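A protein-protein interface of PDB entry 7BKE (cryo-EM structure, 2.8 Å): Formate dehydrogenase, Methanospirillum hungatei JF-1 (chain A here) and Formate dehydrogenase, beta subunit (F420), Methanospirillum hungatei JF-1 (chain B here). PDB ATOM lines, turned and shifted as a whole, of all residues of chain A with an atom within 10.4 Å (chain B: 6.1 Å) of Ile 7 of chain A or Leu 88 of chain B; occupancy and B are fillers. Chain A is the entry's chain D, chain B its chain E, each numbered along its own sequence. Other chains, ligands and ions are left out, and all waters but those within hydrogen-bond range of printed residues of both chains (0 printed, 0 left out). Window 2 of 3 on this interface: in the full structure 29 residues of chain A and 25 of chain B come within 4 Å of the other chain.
The side-chain hydroxyl of Tyr 87 of chain B is in hydrogen-bond range of the side-chain carboxylate of Glu 37 of chain A (2.6 Å).
The backbone NH (N) of Val 34 of chain A lies within hydrogen-bond range of the backbone carbonyl oxygen (O) of Val 27 of chain A (2.8 Å).
Val 59 of chain B touches Ile 7 of chain A. Leu 88 of chain B touches Ile 7 of chain A. Val 59 of chain B touches Met 8 of chain A. Met 8 of chain A touches Leu 83 of chain B. Leu 83 of chain B touches Tyr 10 of chain A (CD1 to OH, 3.3 Å). CZ of Tyr 87 of chain B touches CG2 of Val 27 of chain A, at 3.9 Å. Tyr 87 of chain B touches Val 34 of chain A. Leu 83 of chain B touches Glu 37 of chain A (CD2 to OE2, 3.7 Å).
Ile 7 of chain A touches just these residues of chain B: Val 59 and Leu 88. Of the printed residues of chain B, Met 8 of chain A touches Val 59 and Leu 83. Asn 30 of chain A touches none of the printed residues of chain B. Of the printed residues of chain A, Tyr 87 of chain B touches Val 27 (3.9 Å), Val 34 (3.5 Å) and Glu 37 (2.6 Å). Leu 88 of chain B touches just one residue of chain A: Ile 7 (3.5 Å). No residue of chain A comes within 4 Å of Asn 89 of chain B. No residue of chain A comes within 4 Å of Gly 90 of chain B. No residue of chain A comes within 4 Å of Ala 91 of chain B. The nearest residue of chain A that does not touch Leu 88 of chain B is Met 8 of chain A (4.2 Å). The nearest printed residue of chain B that does not touch Met 8 of chain A is Tyr 87 of chain B (4.1 Å).
Printed residues of chain B that touch a printed residue of chain A: Val 59, Leu 83, Tyr 87 and Leu 88. Hydrophobic or aromatic side chains of chain B within 4 Å of the printed part of chain A: Val 59, Leu 83, Tyr 87 and Leu 88. Among the printed residues, 9 pairs touch across the chains. Among the printed residues, no Asp or Glu carboxylate lies within 4 Å of a Lys or Arg side-chain nitrogen of the other chain.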
ATOM      1  N   SER A   5     -13.057  32.234  20.127  1.00  0.00           N
ATOM      2  CA  SER A   5     -12.089  33.264  20.477  1.00  0.00           C
ATOM      3  C   SER A   5     -10.742  33.004  19.826  1.00  0.00           C
ATOM      4  O   SER A   5     -10.439  33.534  18.760  1.00  0.00           O
ATOM      5  CB  SER A   5     -11.921  33.354  22.000  1.00  0.00           C
ATOM      6  OG  SER A   5     -13.053  33.950  22.611  1.00  0.00           O
ATOM      7  N   GLU A   6      -9.941  32.175  20.486  1.00  0.00           N
ATOM      8  CA  GLU A   6      -8.574  31.888  20.087  1.00  0.00           C
ATOM      9  C   GLU A   6      -8.398  30.383  19.976  1.00  0.00           C
ATOM     10  O   GLU A   6      -8.881  29.636  20.833  1.00  0.00           O
ATOM     11  CB  GLU A   6      -7.593  32.468  21.106  1.00  0.00           C
ATOM     12  CG  GLU A   6      -7.881  32.000  22.521  1.00  0.00           C
ATOM     13  CD  GLU A   6      -7.356  32.937  23.578  1.00  0.00           C
ATOM     14  OE1 GLU A   6      -6.832  34.010  23.223  1.00  0.00           O
ATOM     15  OE2 GLU A   6      -7.489  32.606  24.773  1.00  0.00           O
ATOM     16  N   ILE A   7      -7.728  29.940  18.919  1.00  0.00           N
ATOM     17  CA  ILE A   7      -7.425  28.531  18.715  1.00  0.00           C
ATOM     18  C   ILE A   7      -5.915  28.374  18.676  1.00  0.00           C
ATOM     19  O   ILE A   7      -5.252  28.954  17.813  1.00  0.00           O
ATOM     20  CB  ILE A   7      -8.061  27.985  17.428  1.00  0.00           C
ATOM     21  CG1 ILE A   7      -9.582  28.047  17.505  1.00  0.00           C
ATOM     22  CG2 ILE A   7      -7.621  26.562  17.193  1.00  0.00           C
ATOM     23  CD1 ILE A   7     -10.178  29.251  16.827  1.00  0.00           C
ATOM     24  N   MET A   8      -5.375  27.572  19.587  1.00  0.00           N
ATOM     25  CA  MET A   8      -3.923  27.278  19.611  1.00  0.00           C
ATOM     26  C   MET A   8      -3.143  28.572  19.611  1.00  0.00           C
ATOM     27  O   MET A   8      -2.527  28.879  18.604  1.00  0.00           O
ATOM     28  CB  MET A   8      -3.465  26.380  18.456  1.00  0.00           C
ATOM     29  CG  MET A   8      -2.115  25.738  18.704  1.00  0.00           C
ATOM     30  SD  MET A   8      -1.386  24.916  17.270  1.00  0.00           S
ATOM     31  CE  MET A   8      -0.894  26.324  16.278  1.00  0.00           C
ATOM     32  N   LYS A   9      -3.205  29.317  20.690  1.00  0.00           N
ATOM     33  CA  LYS A   9      -2.393  30.508  20.854  1.00  0.00           C
ATOM     34  C   LYS A   9      -1.222  30.188  21.766  1.00  0.00           C
ATOM     35  O   LYS A   9      -1.395  29.525  22.790  1.00  0.00           O
ATOM     36  CB  LYS A   9      -3.224  31.647  21.423  1.00  0.00           C
ATOM     37  CG  LYS A   9      -2.733  33.016  21.047  1.00  0.00           C
ATOM     38  CD  LYS A   9      -3.582  34.066  21.709  1.00  0.00           C
ATOM     39  CE  LYS A   9      -3.652  33.830  23.202  1.00  0.00           C
ATOM     40  NZ  LYS A   9      -2.375  34.173  23.852  1.00  0.00           N
ATOM     41  N   TYR A  10      -0.038  30.646  21.391  1.00  0.00           N
ATOM     42  CA  TYR A  10       1.189  30.382  22.125  1.00  0.00           C
ATOM     43  C   TYR A  10       1.470  31.531  23.079  1.00  0.00           C
ATOM     44  O   TYR A  10       1.437  32.692  22.672  1.00  0.00           O
ATOM     45  CB  TYR A  10       2.361  30.219  21.161  1.00  0.00           C
ATOM     46  CG  TYR A  10       2.577  28.821  20.656  1.00  0.00           C
ATOM     47  CD1 TYR A  10       3.842  28.272  20.615  1.00  0.00           C
ATOM     48  CD2 TYR A  10       1.523  28.055  20.204  1.00  0.00           C
ATOM     49  CE1 TYR A  10       4.051  27.005  20.157  1.00  0.00           C
ATOM     50  CE2 TYR A  10       1.721  26.781  19.745  1.00  0.00           C
ATOM     51  CZ  TYR A  10       2.988  26.262  19.726  1.00  0.00           C
ATOM     52  OH  TYR A  10       3.193  24.991  19.266  1.00  0.00           O
ATOM     53  N   VAL A  11       1.748  31.212  24.339  1.00  0.00           N
ATOM     54  CA  VAL A  11       2.080  32.208  25.351  1.00  0.00           C
ATOM     55  C   VAL A  11       3.390  31.804  26.001  1.00  0.00           C
ATOM     56  O   VAL A  11       3.484  30.719  26.579  1.00  0.00           O
ATOM     57  CB  VAL A  11       0.981  32.340  26.415  1.00  0.00           C
ATOM     58  CG1 VAL A  11       1.253  33.528  27.300  1.00  0.00           C
ATOM     59  CG2 VAL A  11      -0.374  32.462  25.770  1.00  0.00           C
ATOM     60  N   LEU A  26       2.886  27.987  26.565  1.00  0.00           N
ATOM     61  CA  LEU A  26       1.608  27.385  26.899  1.00  0.00           C
ATOM     62  C   LEU A  26       0.662  27.580  25.727  1.00  0.00           C
ATOM     63  O   LEU A  26       0.591  28.673  25.164  1.00  0.00           O
ATOM     64  CB  LEU A  26       1.026  28.016  28.161  1.00  0.00           C
ATOM     65  CG  LEU A  26       1.807  27.829  29.454  1.00  0.00           C
ATOM     66  CD1 LEU A  26       1.190  28.641  30.550  1.00  0.00           C
ATOM     67  CD2 LEU A  26       1.830  26.379  29.835  1.00  0.00           C
ATOM     68  N   VAL A  27      -0.021  26.506  25.345  1.00  0.00           N
ATOM     69  CA  VAL A  27      -1.004  26.557  24.233  1.00  0.00           C
ATOM     70  C   VAL A  27      -2.363  26.814  24.852  1.00  0.00           C
ATOM     71  O   VAL A  27      -2.721  26.067  25.724  1.00  0.00           O
ATOM     72  CB  VAL A  27      -0.981  25.283  23.385  1.00  0.00           C
ATOM     73  CG1 VAL A  27      -1.893  25.396  22.182  1.00  0.00           C
ATOM     74  CG2 VAL A  27       0.427  24.954  22.945  1.00  0.00           C
ATOM     75  N   VAL A  28      -3.059  27.856  24.430  1.00  0.00           N
ATOM     76  CA  VAL A  28      -4.301  28.289  25.046  1.00  0.00           C
ATOM     77  C   VAL A  28      -5.384  28.276  23.984  1.00  0.00           C
ATOM     78  O   VAL A  28      -5.349  29.083  23.049  1.00  0.00           O
ATOM     79  CB  VAL A  28      -4.160  29.679  25.670  1.00  0.00           C
ATOM     80  CG1 VAL A  28      -5.500  30.215  26.057  1.00  0.00           C
ATOM     81  CG2 VAL A  28      -3.250  29.620  26.862  1.00  0.00           C
ATOM     82  N   SER A  29      -6.357  27.386  24.129  1.00  0.00           N
ATOM     83  CA  SER A  29      -7.451  27.264  23.176  1.00  0.00           C
ATOM     84  C   SER A  29      -8.769  27.505  23.896  1.00  0.00           C
ATOM     85  O   SER A  29      -9.108  26.772  24.827  1.00  0.00           O
ATOM     86  CB  SER A  29      -7.454  25.889  22.522  1.00  0.00           C
ATOM     87  OG  SER A  29      -7.994  24.934  23.410  1.00  0.00           O
ATOM     88  N   ASN A  30      -9.517  28.512  23.443  1.00  0.00           N
ATOM     89  CA  ASN A  30     -10.767  28.930  24.084  1.00  0.00           C
ATOM     90  C   ASN A  30     -10.567  29.201  25.571  1.00  0.00           C
ATOM     91  O   ASN A  30     -11.360  28.773  26.412  1.00  0.00           O
ATOM     92  CB  ASN A  30     -11.877  27.904  23.877  1.00  0.00           C
ATOM     93  CG  ASN A  30     -11.997  27.455  22.447  1.00  0.00           C
ATOM     94  OD1 ASN A  30     -11.798  26.281  22.138  1.00  0.00           O
ATOM     95  ND2 ASN A  30     -12.336  28.381  21.562  1.00  0.00           N
ATOM     96  N   GLY A  31      -9.499  29.913  25.906  1.00  0.00           N
ATOM     97  CA  GLY A  31      -9.273  30.266  27.288  1.00  0.00           C
ATOM     98  C   GLY A  31      -8.961  29.109  28.203  1.00  0.00           C
ATOM     99  O   GLY A  31      -9.166  29.215  29.412  1.00  0.00           O
ATOM    100  N   LYS A  32      -8.478  27.992  27.664  1.00  0.00           N
ATOM    101  CA  LYS A  32      -8.035  26.861  28.464  1.00  0.00           C
ATOM    102  C   LYS A  32      -6.624  26.492  28.041  1.00  0.00           C
ATOM    103  O   LYS A  32      -6.348  26.379  26.847  1.00  0.00           O
ATOM    104  CB  LYS A  32      -8.957  25.651  28.290  1.00  0.00           C
ATOM    105  CG  LYS A  32     -10.427  25.912  28.538  1.00  0.00           C
ATOM    106  CD  LYS A  32     -10.740  26.049  30.015  1.00  0.00           C
ATOM    107  CE  LYS A  32     -10.586  24.725  30.735  1.00  0.00           C
ATOM    108  NZ  LYS A  32     -11.520  23.686  30.240  1.00  0.00           N
ATOM    109  N   VAL A  34      -4.048  24.026  27.135  1.00  0.00           N
ATOM    110  CA  VAL A  34      -4.275  22.660  26.605  1.00  0.00           C
ATOM    111  C   VAL A  34      -2.942  21.958  26.351  1.00  0.00           C
ATOM    112  O   VAL A  34      -2.975  20.806  25.960  1.00  0.00           O
ATOM    113  CB  VAL A  34      -5.157  22.732  25.342  1.00  0.00           C
ATOM    114  CG1 VAL A  34      -6.593  23.067  25.691  1.00  0.00           C
ATOM    115  CG2 VAL A  34      -4.619  23.692  24.301  1.00  0.00           C
ATOM    116  N   GLU A  37       4.465  23.785  24.883  1.00  0.00           N
ATOM    117  CA  GLU A  37       5.209  23.642  23.621  1.00  0.00           C
ATOM    118  C   GLU A  37       6.634  24.152  23.852  1.00  0.00           C
ATOM    119  O   GLU A  37       6.812  24.885  24.821  1.00  0.00           O
ATOM    120  CB  GLU A  37       4.437  24.223  22.457  1.00  0.00           C
ATOM    121  CG  GLU A  37       3.364  23.286  21.940  1.00  0.00           C
ATOM    122  CD  GLU A  37       3.768  21.841  21.690  1.00  0.00           C
ATOM    123  OE1 GLU A  37       2.990  20.940  22.054  1.00  0.00           O
ATOM    124  OE2 GLU A  37       4.849  21.615  21.112  1.00  0.00           O
ATOM    125  N   VAL B  44      -2.736  27.942   8.959  1.00  0.00           N
ATOM    126  CA  VAL B  44      -1.696  27.685   9.943  1.00  0.00           C
ATOM    127  C   VAL B  44      -0.372  28.096   9.317  1.00  0.00           C
ATOM    128  O   VAL B  44       0.256  27.316   8.601  1.00  0.00           O
ATOM    129  CB  VAL B  44      -1.676  26.225  10.388  1.00  0.00           C
ATOM    130  CG1 VAL B  44      -0.685  26.040  11.502  1.00  0.00           C
ATOM    131  CG2 VAL B  44      -3.049  25.811  10.834  1.00  0.00           C
ATOM    132  N   THR B  58       0.835  29.915  14.049  1.00  0.00           N
ATOM    133  CA  THR B  58      -0.343  30.742  14.254  1.00  0.00           C
ATOM    134  C   THR B  58      -1.502  30.219  13.430  1.00  0.00           C
ATOM    135  O   THR B  58      -1.363  30.031  12.221  1.00  0.00           O
ATOM    136  CB  THR B  58      -0.050  32.192  13.874  1.00  0.00           C
ATOM    137  OG1 THR B  58       1.032  32.680  14.672  1.00  0.00           O
ATOM    138  CG2 THR B  58      -1.255  33.063  14.118  1.00  0.00           C
ATOM    139  N   VAL B  59      -2.637  29.993  14.077  1.00  0.00           N
ATOM    140  CA  VAL B  59      -3.883  29.714  13.377  1.00  0.00           C
ATOM    141  C   VAL B  59      -4.588  31.040  13.168  1.00  0.00           C
ATOM    142  O   VAL B  59      -4.855  31.768  14.125  1.00  0.00           O
ATOM    143  CB  VAL B  59      -4.762  28.736  14.164  1.00  0.00           C
ATOM    144  CG1 VAL B  59      -6.080  28.556  13.475  1.00  0.00           C
ATOM    145  CG2 VAL B  59      -4.072  27.414  14.306  1.00  0.00           C
ATOM    146  N   THR B  61      -7.776  33.149  11.376  1.00  0.00           N
ATOM    147  CA  THR B  61      -9.096  33.122  10.774  1.00  0.00           C
ATOM    148  C   THR B  61      -9.506  34.467  10.193  1.00  0.00           C
ATOM    149  O   THR B  61     -10.272  34.501   9.230  1.00  0.00           O
ATOM    150  CB  THR B  61     -10.130  32.663  11.805  1.00  0.00           C
ATOM    151  OG1 THR B  61      -9.780  31.354  12.266  1.00  0.00           O
ATOM    152  CG2 THR B  61     -11.511  32.588  11.186  1.00  0.00           C
ATOM    153  N   LEU B  83       1.285  19.553  15.627  1.00  0.00           N
ATOM    154  CA  LEU B  83       0.432  20.542  16.353  1.00  0.00           C
ATOM    155  C   LEU B  83      -1.023  20.486  15.878  1.00  0.00           C
ATOM    156  O   LEU B  83      -1.901  20.667  16.698  1.00  0.00           O
ATOM    157  CB  LEU B  83       1.037  21.936  16.218  1.00  0.00           C
ATOM    158  CG  LEU B  83       2.502  22.053  16.613  1.00  0.00           C
ATOM    159  CD1 LEU B  83       3.027  23.441  16.303  1.00  0.00           C
ATOM    160  CD2 LEU B  83       2.698  21.713  18.081  1.00  0.00           C
ATOM    161  N   ILE B  84      -1.259  20.280  14.589  1.00  0.00           N
ATOM    162  CA  ILE B  84      -2.629  20.155  14.026  1.00  0.00           C
ATOM    163  C   ILE B  84      -3.316  18.919  14.598  1.00  0.00           C
ATOM    164  O   ILE B  84      -4.476  19.017  14.909  1.00  0.00           O
ATOM    165  CB  ILE B  84      -2.596  20.163  12.489  1.00  0.00           C
ATOM    166  CG1 ILE B  84      -2.048  21.485  11.957  1.00  0.00           C
ATOM    167  CG2 ILE B  84      -3.954  19.840  11.896  1.00  0.00           C
ATOM    168  CD1 ILE B  84      -1.688  21.446  10.504  1.00  0.00           C
ATOM    169  N   LYS B  85      -2.635  17.800  14.752  1.00  0.00           N
ATOM    170  CA  LYS B  85      -3.252  16.612  15.378  1.00  0.00           C
ATOM    171  C   LYS B  85      -3.584  16.873  16.848  1.00  0.00           C
ATOM    172  O   LYS B  85      -4.702  16.575  17.240  1.00  0.00           O
ATOM    173  CB  LYS B  85      -2.301  15.429  15.193  1.00  0.00           C
ATOM    174  CG  LYS B  85      -2.587  14.185  16.017  1.00  0.00           C
ATOM    175  CD  LYS B  85      -1.329  13.563  16.567  1.00  0.00           C
ATOM    176  CE  LYS B  85      -1.588  12.309  17.373  1.00  0.00           C
ATOM    177  NZ  LYS B  85      -0.608  12.148  18.470  1.00  0.00           N
ATOM    178  N   LYS B  86      -2.663  17.424  17.627  1.00  0.00           N
ATOM    179  CA  LYS B  86      -2.846  17.628  19.079  1.00  0.00           C
ATOM    180  C   LYS B  86      -3.855  18.706  19.452  1.00  0.00           C
ATOM    181  O   LYS B  86      -4.625  18.458  20.367  1.00  0.00           O
ATOM    182  CB  LYS B  86      -1.502  17.990  19.700  1.00  0.00           C
ATOM    183  CG  LYS B  86      -0.431  16.914  19.720  1.00  0.00           C
ATOM    184  CD  LYS B  86       0.821  17.405  20.407  1.00  0.00           C
ATOM    185  CE  LYS B  86       1.985  16.442  20.312  1.00  0.00           C
ATOM    186  NZ  LYS B  86       1.934  15.400  21.365  1.00  0.00           N
ATOM    187  N   TYR B  87      -3.845  19.865  18.807  1.00  0.00           N
ATOM    188  CA  TYR B  87      -4.691  21.000  19.243  1.00  0.00           C
ATOM    189  C   TYR B  87      -5.704  21.469  18.192  1.00  0.00           C
ATOM    190  O   TYR B  87      -6.388  22.440  18.466  1.00  0.00           O
ATOM    191  CB  TYR B  87      -3.798  22.160  19.672  1.00  0.00           C
ATOM    192  CG  TYR B  87      -2.635  21.823  20.562  1.00  0.00           C
ATOM    193  CD1 TYR B  87      -2.834  21.407  21.861  1.00  0.00           C
ATOM    194  CD2 TYR B  87      -1.336  21.956  20.110  1.00  0.00           C
ATOM    195  CE1 TYR B  87      -1.769  21.098  22.684  1.00  0.00           C
ATOM    196  CE2 TYR B  87      -0.259  21.657  20.921  1.00  0.00           C
ATOM    197  CZ  TYR B  87      -0.478  21.228  22.213  1.00  0.00           C
ATOM    198  OH  TYR B  87       0.573  20.928  23.026  1.00  0.00           O
ATOM    199  N   LEU B  88      -5.795  20.843  17.035  1.00  0.00           N
ATOM    200  CA  LEU B  88      -6.824  21.204  16.026  1.00  0.00           C
ATOM    201  C   LEU B  88      -7.610  19.955  15.653  1.00  0.00           C
ATOM    202  O   LEU B  88      -8.150  19.942  14.547  1.00  0.00           O
ATOM    203  CB  LEU B  88      -6.185  21.833  14.784  1.00  0.00           C
ATOM    204  CG  LEU B  88      -6.246  23.346  14.633  1.00  0.00           C
ATOM    205  CD1 LEU B  88      -7.616  23.865  15.015  1.00  0.00           C
ATOM    206  CD2 LEU B  88      -5.154  24.016  15.444  1.00  0.00           C
ATOM    207  N   ASN B  89      -7.631  18.945  16.517  1.00  0.00           N
ATOM    208  CA  ASN B  89      -8.408  17.696  16.294  1.00  0.00           C
ATOM    209  C   ASN B  89      -8.067  17.069  14.952  1.00  0.00           C
ATOM    210  O   ASN B  89      -8.963  16.521  14.333  1.00  0.00           O
ATOM    211  CB  ASN B  89      -9.913  17.881  16.459  1.00  0.00           C
ATOM    212  CG  ASN B  89     -10.663  16.616  16.809  1.00  0.00           C
ATOM    213  OD1 ASN B  89     -10.097  15.685  17.374  1.00  0.00           O
ATOM    214  ND2 ASN B  89     -11.939  16.576  16.467  1.00  0.00           N
ATOM    215  N   GLY B  90      -6.821  17.153  14.522  1.00  0.00           N
ATOM    216  CA  GLY B  90      -6.432  16.446  13.323  1.00  0.00           C
ATOM    217  C   GLY B  90      -7.108  16.923  12.069  1.00  0.00           C
ATOM    218  O   GLY B  90      -7.123  16.195  11.078  1.00  0.00           O
ATOM    219  N   ALA B  91      -7.673  18.126  12.083  1.00  0.00           N
ATOM    220  CA  ALA B  91      -8.361  18.692  10.927  1.00  0.00           C
ATOM    221  C   ALA B  91      -9.448  17.756  10.420  1.00  0.00           C
ATOM    222  O   ALA B  91      -9.665  17.617   9.217  1.00  0.00           O
ATOM    223  CB  ALA B  91      -7.377  19.030   9.811  1.00  0.00           C
ATOM    224  N   LYS B  92     -10.146  17.109  11.350  1.00  0.00           N
ATOM    225  CA  LYS B  92     -11.180  16.155  10.979  1.00  0.00           C
ATOM    226  C   LYS B  92     -12.506  16.817  10.656  1.00  0.00           C
ATOM    227  O   LYS B  92     -13.338  16.208   9.980  1.00  0.00           O
ATOM    228  CB  LYS B  92     -11.373  15.130  12.093  1.00  0.00           C
ATOM    229  CG  LYS B  92     -10.339  14.034  12.059  1.00  0.00           C
ATOM    230  CD  LYS B  92     -10.278  13.260  13.357  1.00  0.00           C
ATOM    231  CE  LYS B  92      -8.953  12.531  13.464  1.00  0.00           C
ATOM    232  NZ  LYS B  92      -8.619  11.843  12.188  1.00  0.00           N
ATOM    233  N   ASP B  93     -12.719  18.048  11.109  1.00  0.00           N
ATOM    234  CA  ASP B  93     -13.959  18.759  10.853  1.00  0.00           C
ATOM    235  C   ASP B  93     -13.786  20.065  10.097  1.00  0.00           C
ATOM    236  O   ASP B  93     -14.752  20.527   9.479  1.00  0.00           O
ATOM    237  CB  ASP B  93     -14.681  19.056  12.172  1.00  0.00           C
ATOM    238  CG  ASP B  93     -13.789  19.749  13.169  1.00  0.00           C
ATOM    239  OD1 ASP B  93     -12.574  19.463  13.167  1.00  0.00           O
ATOM    240  OD2 ASP B  93     -14.296  20.587  13.944  1.00  0.00           O
ATOM    241  N   MET B  94     -12.608  20.671  10.120  1.00  0.00           N
ATOM    242  CA  MET B  94     -12.389  21.974   9.519  1.00  0.00           C
ATOM    243  C   MET B  94     -11.309  21.889   8.455  1.00  0.00           C
ATOM    244  O   MET B  94     -10.300  21.203   8.637  1.00  0.00           O
ATOM    245  CB  MET B  94     -12.004  23.001  10.587  1.00  0.00           C
ATOM    246  CG  MET B  94     -10.636  22.808  11.196  1.00  0.00           C
ATOM    247  SD  MET B  94     -10.430  23.801  12.676  1.00  0.00           S
ATOM    248  CE  MET B  94     -10.571  25.448  11.993  1.00  0.00           C
ATOM    249  N   LEU B  96      -8.215  23.414   6.465  1.00  0.00           N
ATOM    250  CA  LEU B  96      -7.092  24.289   6.748  1.00  0.00           C
ATOM    251  C   LEU B  96      -6.262  24.455   5.491  1.00  0.00           C
ATOM    252  O   LEU B  96      -6.314  23.627   4.584  1.00  0.00           O
ATOM    253  CB  LEU B  96      -6.202  23.743   7.857  1.00  0.00           C
ATOM    254  CG  LEU B  96      -6.858  23.304   9.155  1.00  0.00           C
ATOM    255  CD1 LEU B  96      -5.819  22.757  10.088  1.00  0.00           C
ATOM    256  CD2 LEU B  96      -7.556  24.463   9.789  1.00  0.00           C
